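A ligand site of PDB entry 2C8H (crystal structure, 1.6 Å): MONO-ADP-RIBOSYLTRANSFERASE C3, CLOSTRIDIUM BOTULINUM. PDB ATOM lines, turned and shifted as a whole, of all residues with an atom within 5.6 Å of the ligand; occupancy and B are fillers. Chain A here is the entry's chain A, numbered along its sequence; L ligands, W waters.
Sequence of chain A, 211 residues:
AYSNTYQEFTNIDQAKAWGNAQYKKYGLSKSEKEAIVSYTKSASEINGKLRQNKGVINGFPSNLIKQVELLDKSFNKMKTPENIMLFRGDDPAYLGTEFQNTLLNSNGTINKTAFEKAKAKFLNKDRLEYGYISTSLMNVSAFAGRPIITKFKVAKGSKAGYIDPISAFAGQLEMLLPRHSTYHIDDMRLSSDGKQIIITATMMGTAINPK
O13 of the ligand sits at hydrogen-bond distance from OE1 of Glu 174 (2.5 Å).
An oxygen (O12) of the ligand is in hydrogen-bond range of the backbone carbonyl oxygen of Thr 40 (2.7 Å).
OD1 of Asp 90 sits at hydrogen-bond distance from O6 of the ligand, 2.8 Å away.
O1 of the ligand lies within salt-bridge range of NH2 of Arg 88, at 2.8 Å.
An oxygen (O9) of the ligand is in salt-bridge range of the guanidinium group of Arg 146 (2.9 Å).
O6 of the ligand is in hydrogen-bond range of N of Asp 91 (2.9 Å).
O5 of the ligand sits at hydrogen-bond distance from OD2 of Asp 91 (3.4 Å).
An oxygen (O14) of the ligand sits at hydrogen-bond distance from the backbone NH of Gly 89, at 3.0 Å.
O of Gly 89 is in hydrogen-bond range of N7 of the ligand, at 3.1 Å.
The side-chain amide nitrogen (ND2) of Asn 47 sits at hydrogen-bond distance from an oxygen (O2) of the ligand, at 3.1 Å.
The guanidinium group of Arg 51 lies within salt-bridge range of an oxygen (O2) of the ligand, at 3.1 Å.
A nitrogen (N3) of the ligand sits at hydrogen-bond distance from the side-chain carboxylate of Glu 129, at 3.2 Å.
The side-chain carboxylate (OD2) of Asp 90 lies within salt-bridge range of the guanidinium group (NE) of Arg 88.
The guanidinium group (NH1) of Arg 88 lies within hydrogen-bond range of the backbone carbonyl oxygen (O) of Ser 134 (2.8 Å).
The guanidinium group (NE) of Arg 146 is in salt-bridge range of the side-chain carboxylate (OD1) of Asp 91 (3.9 Å).
The guanidinium group (NH2) of Arg 146 sits at hydrogen-bond distance from the backbone carbonyl oxygen (O) of Gly 89 (3.1 Å).
The side-chain amide nitrogen (ND2) of Asn 47 sits at hydrogen-bond distance from the backbone carbonyl oxygen (O) of Ala 43 (3.3 Å).
NH2 of Arg 127 sits at hydrogen-bond distance from O of Tyr 94, 2.8 Å away.
O of Gln 172 is in hydrogen-bond range of OG of Ser 136, at 2.7 Å.
OH of Tyr 39 is in hydrogen-bond range of OG of Ser 134, 2.8 Å away.
A nitrogen (N5) of the ligand lies close to the backbone carbonyl oxygen (O) of Ala 93 (3.5 Å).
The guanidinium group of Arg 127 lies close to a nitrogen (N3) of the ligand (3.2 Å).
Merely in contact with the ligand: Ala 43 (3.8 Å), Ser 44 (3.7 Å), Tyr 94 (3.8 Å), Ser 134 (3.6 Å), Thr 135 (3.4 Å), Ser 136 (3.4 Å), Phe 143 (3.2 Å) and Gln 172 (3.4 Å).
Hydrophobic or aromatic side chains that line the ligand: Ala 43, Tyr 94 and Phe 143.
Of the 28 residues printed, 20 come within 4 Å of the ligand.
The nearest printed residue that does not touch the ligand is Phe 87 (4.04 Å).
Water W6 bridges OG of Ser 136 (2.9 Å) and O14 of the ligand (2.9 Å).
Water W7 lies within hydrogen-bond range of NE2 of Gln 172 (2.9 Å) and O12 of the ligand (3.0 Å).
Water W8 bridges N2 of the ligand (3.0 Å) and OE1 of Glu 129 (3.2 Å).
Water W4 lies within hydrogen-bond range of the backbone carbonyl oxygen (O) of Tyr 132 (2.7 Å), the guanidinium group (NH1) of Arg 51 (3.0 Å), an oxygen (O1) of the ligand (3.1 Å) and the side-chain carboxylate (OE2) of Glu 129 (3.5 Å).
Water W2 lies within hydrogen-bond range of the guanidinium group (NE) of Arg 127 (3.0 Å), the side-chain carboxylate (OE1) of Glu 129 (3.1 Å) and a nitrogen (N3) of the ligand (3.4 Å).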
ATOM      1  N   TYR A  39      18.630  -6.731  26.671  1.00  0.00           N
ATOM      2  CA  TYR A  39      18.519  -5.927  25.457  1.00  0.00           C
ATOM      3  C   TYR A  39      18.156  -6.800  24.246  1.00  0.00           C
ATOM      4  O   TYR A  39      17.286  -6.433  23.466  1.00  0.00           O
ATOM      5  CB  TYR A  39      19.808  -5.144  25.133  1.00  0.00           C
ATOM      6  CG  TYR A  39      19.754  -4.520  23.754  1.00  0.00           C
ATOM      7  CD1 TYR A  39      19.114  -3.301  23.540  1.00  0.00           C
ATOM      8  CD2 TYR A  39      20.307  -5.168  22.652  1.00  0.00           C
ATOM      9  CE1 TYR A  39      19.038  -2.732  22.269  1.00  0.00           C
ATOM     10  CE2 TYR A  39      20.206  -4.616  21.378  1.00  0.00           C
ATOM     11  CZ  TYR A  39      19.591  -3.402  21.190  1.00  0.00           C
ATOM     12  OH  TYR A  39      19.477  -2.850  19.921  1.00  0.00           O
ATOM     13  N   THR A  40      18.794  -7.956  24.090  1.00  0.00           N
ATOM     14  CA  THR A  40      18.526  -8.795  22.907  1.00  0.00           C
ATOM     15  C   THR A  40      17.095  -9.356  22.927  1.00  0.00           C
ATOM     16  O   THR A  40      16.552  -9.670  21.865  1.00  0.00           O
ATOM     17  CB  THR A  40      19.547  -9.953  22.704  1.00  0.00           C
ATOM     18  OG1 THR A  40      19.467 -10.900  23.776  1.00  0.00           O
ATOM     19  CG2 THR A  40      21.004  -9.432  22.698  1.00  0.00           C
ATOM     20  N   LYS A  41      16.502  -9.483  24.112  1.00  0.00           N
ATOM     21  CA  LYS A  41      15.105  -9.917  24.243  1.00  0.00           C
ATOM     22  C   LYS A  41      14.074  -8.793  24.088  1.00  0.00           C
ATOM     23  O   LYS A  41      12.899  -9.057  23.805  1.00  0.00           O
ATOM     24  CB  LYS A  41      14.883 -10.563  25.616  1.00  0.00           C
ATOM     25  CG  LYS A  41      15.727 -11.789  25.892  1.00  0.00           C
ATOM     26  CD  LYS A  41      15.448 -12.322  27.298  1.00  0.00           C
ATOM     27  CE  LYS A  41      16.427 -13.393  27.706  1.00  0.00           C
ATOM     28  NZ  LYS A  41      16.001 -14.045  28.983  1.00  0.00           N
ATOM     29  N   ALA A  43      14.857  -5.356  22.612  1.00  0.00           N
ATOM     30  CA  ALA A  43      15.474  -4.239  21.894  1.00  0.00           C
ATOM     31  C   ALA A  43      14.449  -3.292  21.242  1.00  0.00           C
ATOM     32  O   ALA A  43      14.567  -2.078  21.364  1.00  0.00           O
ATOM     33  CB  ALA A  43      16.448  -4.744  20.841  1.00  0.00           C
ATOM     34  N   SER A  44      13.457  -3.847  20.563  1.00  0.00           N
ATOM     35  CA  SER A  44      12.470  -3.020  19.869  1.00  0.00           C
ATOM     36  C   SER A  44      11.749  -2.070  20.830  1.00  0.00           C
ATOM     37  O   SER A  44      11.489  -0.921  20.487  1.00  0.00           O
ATOM     38  CB  SER A  44      11.432  -3.894  19.155  1.00  0.00           C
ATOM     39  OG  SER A  44      10.640  -3.108  18.265  1.00  0.00           O
ATOM     40  N   ASN A  47      14.511   0.615  22.260  1.00  0.00           N
ATOM     41  CA  ASN A  47      14.824   1.574  21.203  1.00  0.00           C
ATOM     42  C   ASN A  47      13.632   2.434  20.840  1.00  0.00           C
ATOM     43  O   ASN A  47      13.786   3.609  20.546  1.00  0.00           O
ATOM     44  CB  ASN A  47      15.358   0.837  19.961  1.00  0.00           C
ATOM     45  CG  ASN A  47      16.704   0.162  20.206  1.00  0.00           C
ATOM     46  OD1 ASN A  47      17.498   0.627  21.032  1.00  0.00           O
ATOM     47  ND2 ASN A  47      16.968  -0.927  19.498  1.00  0.00           N
ATOM     48  N   GLY A  48      12.428   1.857  20.883  1.00  0.00           N
ATOM     49  CA  GLY A  48      11.205   2.572  20.596  1.00  0.00           C
ATOM     50  C   GLY A  48      10.964   3.685  21.601  1.00  0.00           C
ATOM     51  O   GLY A  48      10.564   4.777  21.218  1.00  0.00           O
ATOM     52  N   ARG A  51      13.479   6.511  20.994  1.00  0.00           N
ATOM     53  CA  ARG A  51      13.076   7.322  19.848  1.00  0.00           C
ATOM     54  C   ARG A  51      11.930   8.267  20.189  1.00  0.00           C
ATOM     55  O   ARG A  51      11.936   9.440  19.808  1.00  0.00           O
ATOM     56  CB  ARG A  51      12.667   6.424  18.661  1.00  0.00           C
ATOM     57  CG  ARG A  51      13.848   5.755  17.954  1.00  0.00           C
ATOM     58  CD  ARG A  51      13.506   5.100  16.632  1.00  0.00           C
ATOM     59  NE  ARG A  51      12.966   3.743  16.812  1.00  0.00           N
ATOM     60  CZ  ARG A  51      13.692   2.644  16.938  1.00  0.00           C
ATOM     61  NH1 ARG A  51      15.025   2.675  16.911  1.00  0.00           N
ATOM     62  NH2 ARG A  51      13.074   1.478  17.086  1.00  0.00           N
ATOM     63  N   PHE A  87      26.397  -5.053   9.007  1.00  0.00           N
ATOM     64  CA  PHE A  87      25.190  -5.183   8.186  1.00  0.00           C
ATOM     65  C   PHE A  87      23.918  -5.112   9.013  1.00  0.00           C
ATOM     66  O   PHE A  87      23.875  -5.588  10.137  1.00  0.00           O
ATOM     67  CB  PHE A  87      25.221  -6.507   7.414  1.00  0.00           C
ATOM     68  CG  PHE A  87      26.373  -6.616   6.477  1.00  0.00           C
ATOM     69  CD1 PHE A  87      26.245  -6.212   5.152  1.00  0.00           C
ATOM     70  CD2 PHE A  87      27.598  -7.091   6.913  1.00  0.00           C
ATOM     71  CE1 PHE A  87      27.322  -6.293   4.273  1.00  0.00           C
ATOM     72  CE2 PHE A  87      28.683  -7.183   6.036  1.00  0.00           C
ATOM     73  CZ  PHE A  87      28.533  -6.784   4.715  1.00  0.00           C
ATOM     74  N   ARG A  88      22.873  -4.554   8.421  1.00  0.00           N
ATOM     75  CA  ARG A  88      21.615  -4.394   9.115  1.00  0.00           C
ATOM     76  C   ARG A  88      20.432  -4.503   8.174  1.00  0.00           C
ATOM     77  O   ARG A  88      20.500  -4.010   7.053  1.00  0.00           O
ATOM     78  CB  ARG A  88      21.602  -3.029   9.808  1.00  0.00           C
ATOM     79  CG  ARG A  88      20.560  -2.900  10.832  1.00  0.00           C
ATOM     80  CD  ARG A  88      20.484  -1.537  11.458  1.00  0.00           C
ATOM     81  NE  ARG A  88      19.098  -1.253  11.778  1.00  0.00           N
ATOM     82  CZ  ARG A  88      18.464  -1.728  12.844  1.00  0.00           C
ATOM     83  NH1 ARG A  88      19.100  -2.451  13.756  1.00  0.00           N
ATOM     84  NH2 ARG A  88      17.186  -1.433  13.009  1.00  0.00           N
ATOM     85  N   GLY A  89      19.367  -5.169   8.611  1.00  0.00           N
ATOM     86  CA  GLY A  89      18.097  -5.187   7.887  1.00  0.00           C
ATOM     87  C   GLY A  89      17.053  -4.304   8.564  1.00  0.00           C
ATOM     88  O   GLY A  89      16.936  -4.314   9.788  1.00  0.00           O
ATOM     89  N   ASP A  90      16.329  -3.525   7.771  1.00  0.00           N
ATOM     90  CA  ASP A  90      15.246  -2.664   8.272  1.00  0.00           C
ATOM     91  C   ASP A  90      13.956  -2.854   7.478  1.00  0.00           C
ATOM     92  O   ASP A  90      13.987  -3.186   6.293  1.00  0.00           O
ATOM     93  CB  ASP A  90      15.659  -1.193   8.200  1.00  0.00           C
ATOM     94  CG  ASP A  90      16.498  -0.763   9.387  1.00  0.00           C
ATOM     95  OD1 ASP A  90      15.926  -0.567  10.482  1.00  0.00           O
ATOM     96  OD2 ASP A  90      17.737  -0.588   9.313  1.00  0.00           O
ATOM     97  N   ASP A  91      12.828  -2.629   8.145  1.00  0.00           N
ATOM     98  CA  ASP A  91      11.513  -2.612   7.497  1.00  0.00           C
ATOM     99  C   ASP A  91      11.182  -1.193   7.009  1.00  0.00           C
ATOM    100  O   ASP A  91      11.932  -0.257   7.301  1.00  0.00           O
ATOM    101  CB  ASP A  91      10.453  -3.140   8.463  1.00  0.00           C
ATOM    102  CG  ASP A  91      10.565  -4.639   8.685  1.00  0.00           C
ATOM    103  OD1 ASP A  91      11.050  -5.360   7.771  1.00  0.00           O
ATOM    104  OD2 ASP A  91      10.189  -5.186   9.739  1.00  0.00           O
ATOM    105  N   PRO A  92      10.104  -1.005   6.244  1.00  0.00           N
ATOM    106  CA  PRO A  92       9.838   0.292   5.589  1.00  0.00           C
ATOM    107  C   PRO A  92       9.727   1.512   6.520  1.00  0.00           C
ATOM    108  O   PRO A  92      10.120   2.608   6.091  1.00  0.00           O
ATOM    109  CB  PRO A  92       8.521   0.043   4.852  1.00  0.00           C
ATOM    110  CG  PRO A  92       8.520  -1.426   4.594  1.00  0.00           C
ATOM    111  CD  PRO A  92       9.066  -1.989   5.882  1.00  0.00           C
ATOM    112  N   ALA A  93       9.216   1.332   7.729  1.00  0.00           N
ATOM    113  CA  ALA A  93       9.049   2.435   8.689  1.00  0.00           C
ATOM    114  C   ALA A  93      10.370   3.111   9.060  1.00  0.00           C
ATOM    115  O   ALA A  93      10.375   4.253   9.534  1.00  0.00           O
ATOM    116  CB  ALA A  93       8.365   1.950   9.941  1.00  0.00           C
ATOM    117  N   TYR A  94      11.482   2.408   8.854  1.00  0.00           N
ATOM    118  CA  TYR A  94      12.810   2.979   9.040  1.00  0.00           C
ATOM    119  C   TYR A  94      12.968   4.284   8.243  1.00  0.00           C
ATOM    120  O   TYR A  94      13.625   5.222   8.706  1.00  0.00           O
ATOM    121  CB  TYR A  94      13.908   1.970   8.659  1.00  0.00           C
ATOM    122  CG  TYR A  94      15.272   2.599   8.495  1.00  0.00           C
ATOM    123  CD1 TYR A  94      16.047   2.921   9.607  1.00  0.00           C
ATOM    124  CD2 TYR A  94      15.764   2.921   7.237  1.00  0.00           C
ATOM    125  CE1 TYR A  94      17.301   3.531   9.455  1.00  0.00           C
ATOM    126  CE2 TYR A  94      16.991   3.536   7.074  1.00  0.00           C
ATOM    127  CZ  TYR A  94      17.757   3.836   8.186  1.00  0.00           C
ATOM    128  OH  TYR A  94      18.977   4.446   8.022  1.00  0.00           O
ATOM    129  N   ARG A 127      22.272  11.222   9.577  1.00  0.00           N
ATOM    130  CA  ARG A 127      21.102  10.720  10.273  1.00  0.00           C
ATOM    131  C   ARG A 127      21.501  10.385  11.701  1.00  0.00           C
ATOM    132  O   ARG A 127      22.513   9.723  11.922  1.00  0.00           O
ATOM    133  CB  ARG A 127      20.568   9.480   9.578  1.00  0.00           C
ATOM    134  CG  ARG A 127      19.408   8.852  10.298  1.00  0.00           C
ATOM    135  CD  ARG A 127      18.526   8.014   9.391  1.00  0.00           C
ATOM    136  NE  ARG A 127      17.516   7.316  10.176  1.00  0.00           N
ATOM    137  CZ  ARG A 127      16.452   6.716   9.654  1.00  0.00           C
ATOM    138  NH1 ARG A 127      16.260   6.694   8.340  1.00  0.00           N
ATOM    139  NH2 ARG A 127      15.593   6.115  10.463  1.00  0.00           N
ATOM    140  N   GLU A 129      20.409   8.476  15.198  1.00  0.00           N
ATOM    141  CA  GLU A 129      19.584   7.405  15.743  1.00  0.00           C
ATOM    142  C   GLU A 129      19.572   7.458  17.273  1.00  0.00           C
ATOM    143  O   GLU A 129      20.615   7.325  17.900  1.00  0.00           O
ATOM    144  CB  GLU A 129      20.135   6.052  15.285  1.00  0.00           C
ATOM    145  CG  GLU A 129      19.352   4.856  15.782  1.00  0.00           C
ATOM    146  CD  GLU A 129      17.875   4.964  15.490  1.00  0.00           C
ATOM    147  OE1 GLU A 129      17.515   5.235  14.331  1.00  0.00           O
ATOM    148  OE2 GLU A 129      17.076   4.787  16.437  1.00  0.00           O
ATOM    149  N   TYR A 132      19.827   2.221  20.266  1.00  0.00           N
ATOM    150  CA  TYR A 132      21.036   1.445  19.965  1.00  0.00           C
ATOM    151  C   TYR A 132      20.861   0.897  18.569  1.00  0.00           C
ATOM    152  O   TYR A 132      19.732   0.775  18.090  1.00  0.00           O
ATOM    153  CB  TYR A 132      21.242   0.306  20.959  1.00  0.00           C
ATOM    154  CG  TYR A 132      21.363   0.788  22.380  1.00  0.00           C
ATOM    155  CD1 TYR A 132      22.596   1.141  22.903  1.00  0.00           C
ATOM    156  CD2 TYR A 132      20.236   0.934  23.182  1.00  0.00           C
ATOM    157  CE1 TYR A 132      22.699   1.632  24.199  1.00  0.00           C
ATOM    158  CE2 TYR A 132      20.331   1.420  24.477  1.00  0.00           C
ATOM    159  CZ  TYR A 132      21.569   1.754  24.973  1.00  0.00           C
ATOM    160  OH  TYR A 132      21.685   2.228  26.265  1.00  0.00           O
ATOM    161  N   SER A 134      21.554  -2.407  16.467  1.00  0.00           N
ATOM    162  CA  SER A 134      21.916  -3.816  16.299  1.00  0.00           C
ATOM    163  C   SER A 134      22.348  -4.071  14.863  1.00  0.00           C
ATOM    164  O   SER A 134      21.628  -3.719  13.921  1.00  0.00           O
ATOM    165  CB  SER A 134      20.715  -4.707  16.607  1.00  0.00           C
ATOM    166  OG  SER A 134      20.337  -4.643  17.971  1.00  0.00           O
ATOM    167  N   THR A 135      23.518  -4.670  14.695  1.00  0.00           N
ATOM    168  CA  THR A 135      24.044  -5.047  13.384  1.00  0.00           C
ATOM    169  C   THR A 135      24.576  -6.476  13.445  1.00  0.00           C
ATOM    170  O   THR A 135      24.594  -7.085  14.509  1.00  0.00           O
ATOM    171  CB  THR A 135      25.160  -4.095  12.921  1.00  0.00           C
ATOM    172  OG1 THR A 135      26.361  -4.339  13.681  1.00  0.00           O
ATOM    173  CG2 THR A 135      24.823  -2.628  13.168  1.00  0.00           C
ATOM    174  N   SER A 136      25.012  -6.979  12.293  1.00  0.00           N
ATOM    175  CA  SER A 136      25.593  -8.309  12.190  1.00  0.00           C
ATOM    176  C   SER A 136      26.908  -8.239  11.418  1.00  0.00           C
ATOM    177  O   SER A 136      27.093  -7.391  10.556  1.00  0.00           O
ATOM    178  CB  SER A 136      24.630  -9.256  11.464  1.00  0.00           C
ATOM    179  OG  SER A 136      23.407  -9.397  12.169  1.00  0.00           O
ATOM    180  N   PHE A 143      17.416 -11.471   9.224  1.00  0.00           N
ATOM    181  CA  PHE A 143      17.141 -10.091   8.791  1.00  0.00           C
ATOM    182  C   PHE A 143      17.463  -9.772   7.327  1.00  0.00           C
ATOM    183  O   PHE A 143      17.124  -8.682   6.847  1.00  0.00           O
ATOM    184  CB  PHE A 143      17.891  -9.132   9.712  1.00  0.00           C
ATOM    185  CG  PHE A 143      17.655  -9.414  11.158  1.00  0.00           C
ATOM    186  CD1 PHE A 143      16.427  -9.135  11.733  1.00  0.00           C
ATOM    187  CD2 PHE A 143      18.633 -10.010  11.935  1.00  0.00           C
ATOM    188  CE1 PHE A 143      16.182  -9.419  13.056  1.00  0.00           C
ATOM    189  CE2 PHE A 143      18.396 -10.306  13.260  1.00  0.00           C
ATOM    190  CZ  PHE A 143      17.165 -10.004  13.826  1.00  0.00           C
ATOM    191  N   ARG A 146      14.625  -8.559   4.827  1.00  0.00           N
ATOM    192  CA  ARG A 146      13.954  -7.264   4.976  1.00  0.00           C
ATOM    193  C   ARG A 146      14.197  -6.402   3.728  1.00  0.00           C
ATOM    194  O   ARG A 146      15.165  -6.632   3.000  1.00  0.00           O
ATOM    195  CB  ARG A 146      14.450  -6.559   6.240  1.00  0.00           C
ATOM    196  CG  ARG A 146      14.034  -7.263   7.529  1.00  0.00           C
ATOM    197  CD  ARG A 146      14.398  -6.508   8.797  1.00  0.00           C
ATOM    198  NE  ARG A 146      13.742  -7.056   9.973  1.00  0.00           N
ATOM    199  CZ  ARG A 146      13.852  -6.546  11.203  1.00  0.00           C
ATOM    200  NH1 ARG A 146      13.220  -7.105  12.225  1.00  0.00           N
ATOM    201  NH2 ARG A 146      14.601  -5.471  11.413  1.00  0.00           N
ATOM    202  N   SER A 167      23.769 -13.365  23.551  1.00  0.00           N
ATOM    203  CA  SER A 167      22.448 -13.069  23.006  1.00  0.00           C
ATOM    204  C   SER A 167      21.480 -14.197  23.325  1.00  0.00           C
ATOM    205  O   SER A 167      21.869 -15.352  23.430  1.00  0.00           O
ATOM    206  CB  SER A 167      22.499 -12.879  21.487  1.00  0.00           C
ATOM    207  OG  SER A 167      21.202 -12.588  20.967  1.00  0.00           O
ATOM    208  N   PHE A 169      19.272 -15.093  21.235  1.00  0.00           N
ATOM    209  CA  PHE A 169      18.939 -15.655  19.922  1.00  0.00           C
ATOM    210  C   PHE A 169      20.160 -16.160  19.160  1.00  0.00           C
ATOM    211  O   PHE A 169      21.260 -15.594  19.246  1.00  0.00           O
ATOM    212  CB  PHE A 169      18.178 -14.622  19.099  1.00  0.00           C
ATOM    213  CG  PHE A 169      16.872 -14.217  19.710  1.00  0.00           C
ATOM    214  CD1 PHE A 169      15.755 -15.039  19.597  1.00  0.00           C
ATOM    215  CD2 PHE A 169      16.752 -13.034  20.406  1.00  0.00           C
ATOM    216  CE1 PHE A 169      14.553 -14.691  20.172  1.00  0.00           C
ATOM    217  CE2 PHE A 169      15.550 -12.669  20.980  1.00  0.00           C
ATOM    218  CZ  PHE A 169      14.447 -13.491  20.862  1.00  0.00           C
ATOM    219  N   GLN A 172      22.743 -14.813  14.683  1.00  0.00           N
ATOM    220  CA  GLN A 172      22.629 -13.397  14.331  1.00  0.00           C
ATOM    221  C   GLN A 172      23.967 -12.635  14.239  1.00  0.00           C
ATOM    222  O   GLN A 172      24.009 -11.538  13.682  1.00  0.00           O
ATOM    223  CB  GLN A 172      21.649 -12.707  15.283  1.00  0.00           C
ATOM    224  CG  GLN A 172      20.231 -13.252  15.196  1.00  0.00           C
ATOM    225  CD  GLN A 172      19.235 -12.486  16.055  1.00  0.00           C
ATOM    226  OE1 GLN A 172      19.627 -11.598  16.802  1.00  0.00           O
ATOM    227  NE2 GLN A 172      17.958 -12.845  15.956  1.00  0.00           N
ATOM    228  N   GLU A 174      25.719 -10.820  16.201  1.00  0.00           N
ATOM    229  CA  GLU A 174      25.360  -9.437  16.500  1.00  0.00           C
ATOM    230  C   GLU A 174      26.535  -8.608  17.024  1.00  0.00           C
ATOM    231  O   GLU A 174      27.220  -8.999  17.978  1.00  0.00           O
ATOM    232  CB  GLU A 174      24.174  -9.336  17.468  1.00  0.00           C
ATOM    233  CG  GLU A 174      23.892  -7.889  17.883  1.00  0.00           C
ATOM    234  CD  GLU A 174      22.547  -7.665  18.537  1.00  0.00           C
ATOM    235  OE1 GLU A 174      21.836  -8.633  18.850  1.00  0.00           O
ATOM    236  OE2 GLU A 174      22.211  -6.479  18.746  1.00  0.00           O
HETATM  237  P1  LIG L   1      15.050  -1.831  16.163  1.00  0.00           P
HETATM  238  O1  LIG L   1      16.303  -1.250  15.655  1.00  0.00           O
HETATM  239  O2  LIG L   1      14.631  -1.223  17.505  1.00  0.00           O
HETATM  240  O3  LIG L   1      13.916  -1.646  15.052  1.00  0.00           O
HETATM  241  C1  LIG L   1      12.591  -2.110  15.276  1.00  0.00           C
HETATM  242  C2  LIG L   1      11.751  -1.785  14.044  1.00  0.00           C
HETATM  243  O4  LIG L   1      11.732  -0.386  13.822  1.00  0.00           O
HETATM  244  C3  LIG L   1      12.308  -2.392  12.768  1.00  0.00           C
HETATM  245  O5  LIG L   1      11.239  -2.753  11.920  1.00  0.00           O
HETATM  246  C4  LIG L   1      13.144  -1.273  12.163  1.00  0.00           C
HETATM  247  O6  LIG L   1      13.303  -1.367  10.767  1.00  0.00           O
HETATM  248  C5  LIG L   1      12.370  -0.036  12.608  1.00  0.00           C
HETATM  249  N1  LIG L   1      13.196   1.154  12.843  1.00  0.00           N
HETATM  250  C6  LIG L   1      14.535   1.247  13.143  1.00  0.00           C
HETATM  251  N2  LIG L   1      14.865   2.555  13.291  1.00  0.00           N
HETATM  252  C7  LIG L   1      13.749   3.296  13.085  1.00  0.00           C
HETATM  253  C8  LIG L   1      13.518   4.677  13.125  1.00  0.00           C
HETATM  254  N3  LIG L   1      14.519   5.517  13.391  1.00  0.00           N
HETATM  255  N4  LIG L   1      12.251   5.147  12.877  1.00  0.00           N
HETATM  256  C9  LIG L   1      11.216   4.267  12.609  1.00  0.00           C
HETATM  257  N5  LIG L   1      11.458   2.904  12.576  1.00  0.00           N
HETATM  258  C10 LIG L   1      12.701   2.434  12.820  1.00  0.00           C
HETATM  259  O7  LIG L   1      15.172  -3.426  16.343  1.00  0.00           O
HETATM  260  P2  LIG L   1      15.649  -4.455  15.212  1.00  0.00           P
HETATM  261  O8  LIG L   1      17.072  -4.243  14.899  1.00  0.00           O
HETATM  262  O9  LIG L   1      14.622  -4.507  14.156  1.00  0.00           O
HETATM  263  O10 LIG L   1      15.495  -5.822  16.028  1.00  0.00           O
HETATM  264  C11 LIG L   1      16.165  -6.005  17.252  1.00  0.00           C
HETATM  265  C12 LIG L   1      16.300  -7.503  17.492  1.00  0.00           C
HETATM  266  O11 LIG L   1      16.994  -8.134  16.440  1.00  0.00           O
HETATM  267  C13 LIG L   1      17.124  -7.788  18.719  1.00  0.00           C
HETATM  268  O12 LIG L   1      16.693  -9.035  19.210  1.00  0.00           O
HETATM  269  C14 LIG L   1      18.544  -7.803  18.191  1.00  0.00           C
HETATM  270  O13 LIG L   1      19.362  -8.583  19.014  1.00  0.00           O
HETATM  271  C15 LIG L   1      18.327  -8.419  16.814  1.00  0.00           C
HETATM  272  N6  LIG L   1      19.250  -8.058  15.709  1.00  0.00           N
HETATM  273  C16 LIG L   1      18.782  -7.357  14.625  1.00  0.00           C
HETATM  274  C17 LIG L   1      19.623  -7.079  13.555  1.00  0.00           C
HETATM  275  C18 LIG L   1      19.141  -6.304  12.363  1.00  0.00           C
HETATM  276  O14 LIG L   1      20.048  -6.111  11.338  1.00  0.00           O
HETATM  277  N7  LIG L   1      17.897  -5.837  12.255  1.00  0.00           N
HETATM  278  C19 LIG L   1      20.950  -7.495  13.593  1.00  0.00           C
HETATM  279  C20 LIG L   1      21.412  -8.224  14.685  1.00  0.00           C
HETATM  280  C21 LIG L   1      20.549  -8.486  15.736  1.00  0.00           C
HETATM  281  O   HOH W   1       9.126   0.835  13.339  1.00  0.00           O
HETATM  282  O   HOH W   2      16.821   7.985  13.069  1.00  0.00           O
HETATM  283  O   HOH W   3      13.438   8.614  12.496  1.00  0.00           O
HETATM  284  O   HOH W   4      17.723   1.397  16.372  1.00  0.00           O
HETATM  285  O   HOH W   5      18.737  -1.770  16.880  1.00  0.00           O
HETATM  286  O   HOH W   6      21.549  -8.350  10.195  1.00  0.00           O
HETATM  287  O   HOH W   7      15.967 -11.277  17.434  1.00  0.00           O
HETATM  288  O   HOH W   8      17.802   2.141  13.599  1.00  0.00           O
HETATM  289  O   HOH W   9       8.975  -1.280  11.624  1.00  0.00           O
HETATM  290  O   HOH W  10       9.818  -3.964  15.947  1.00  0.00           O
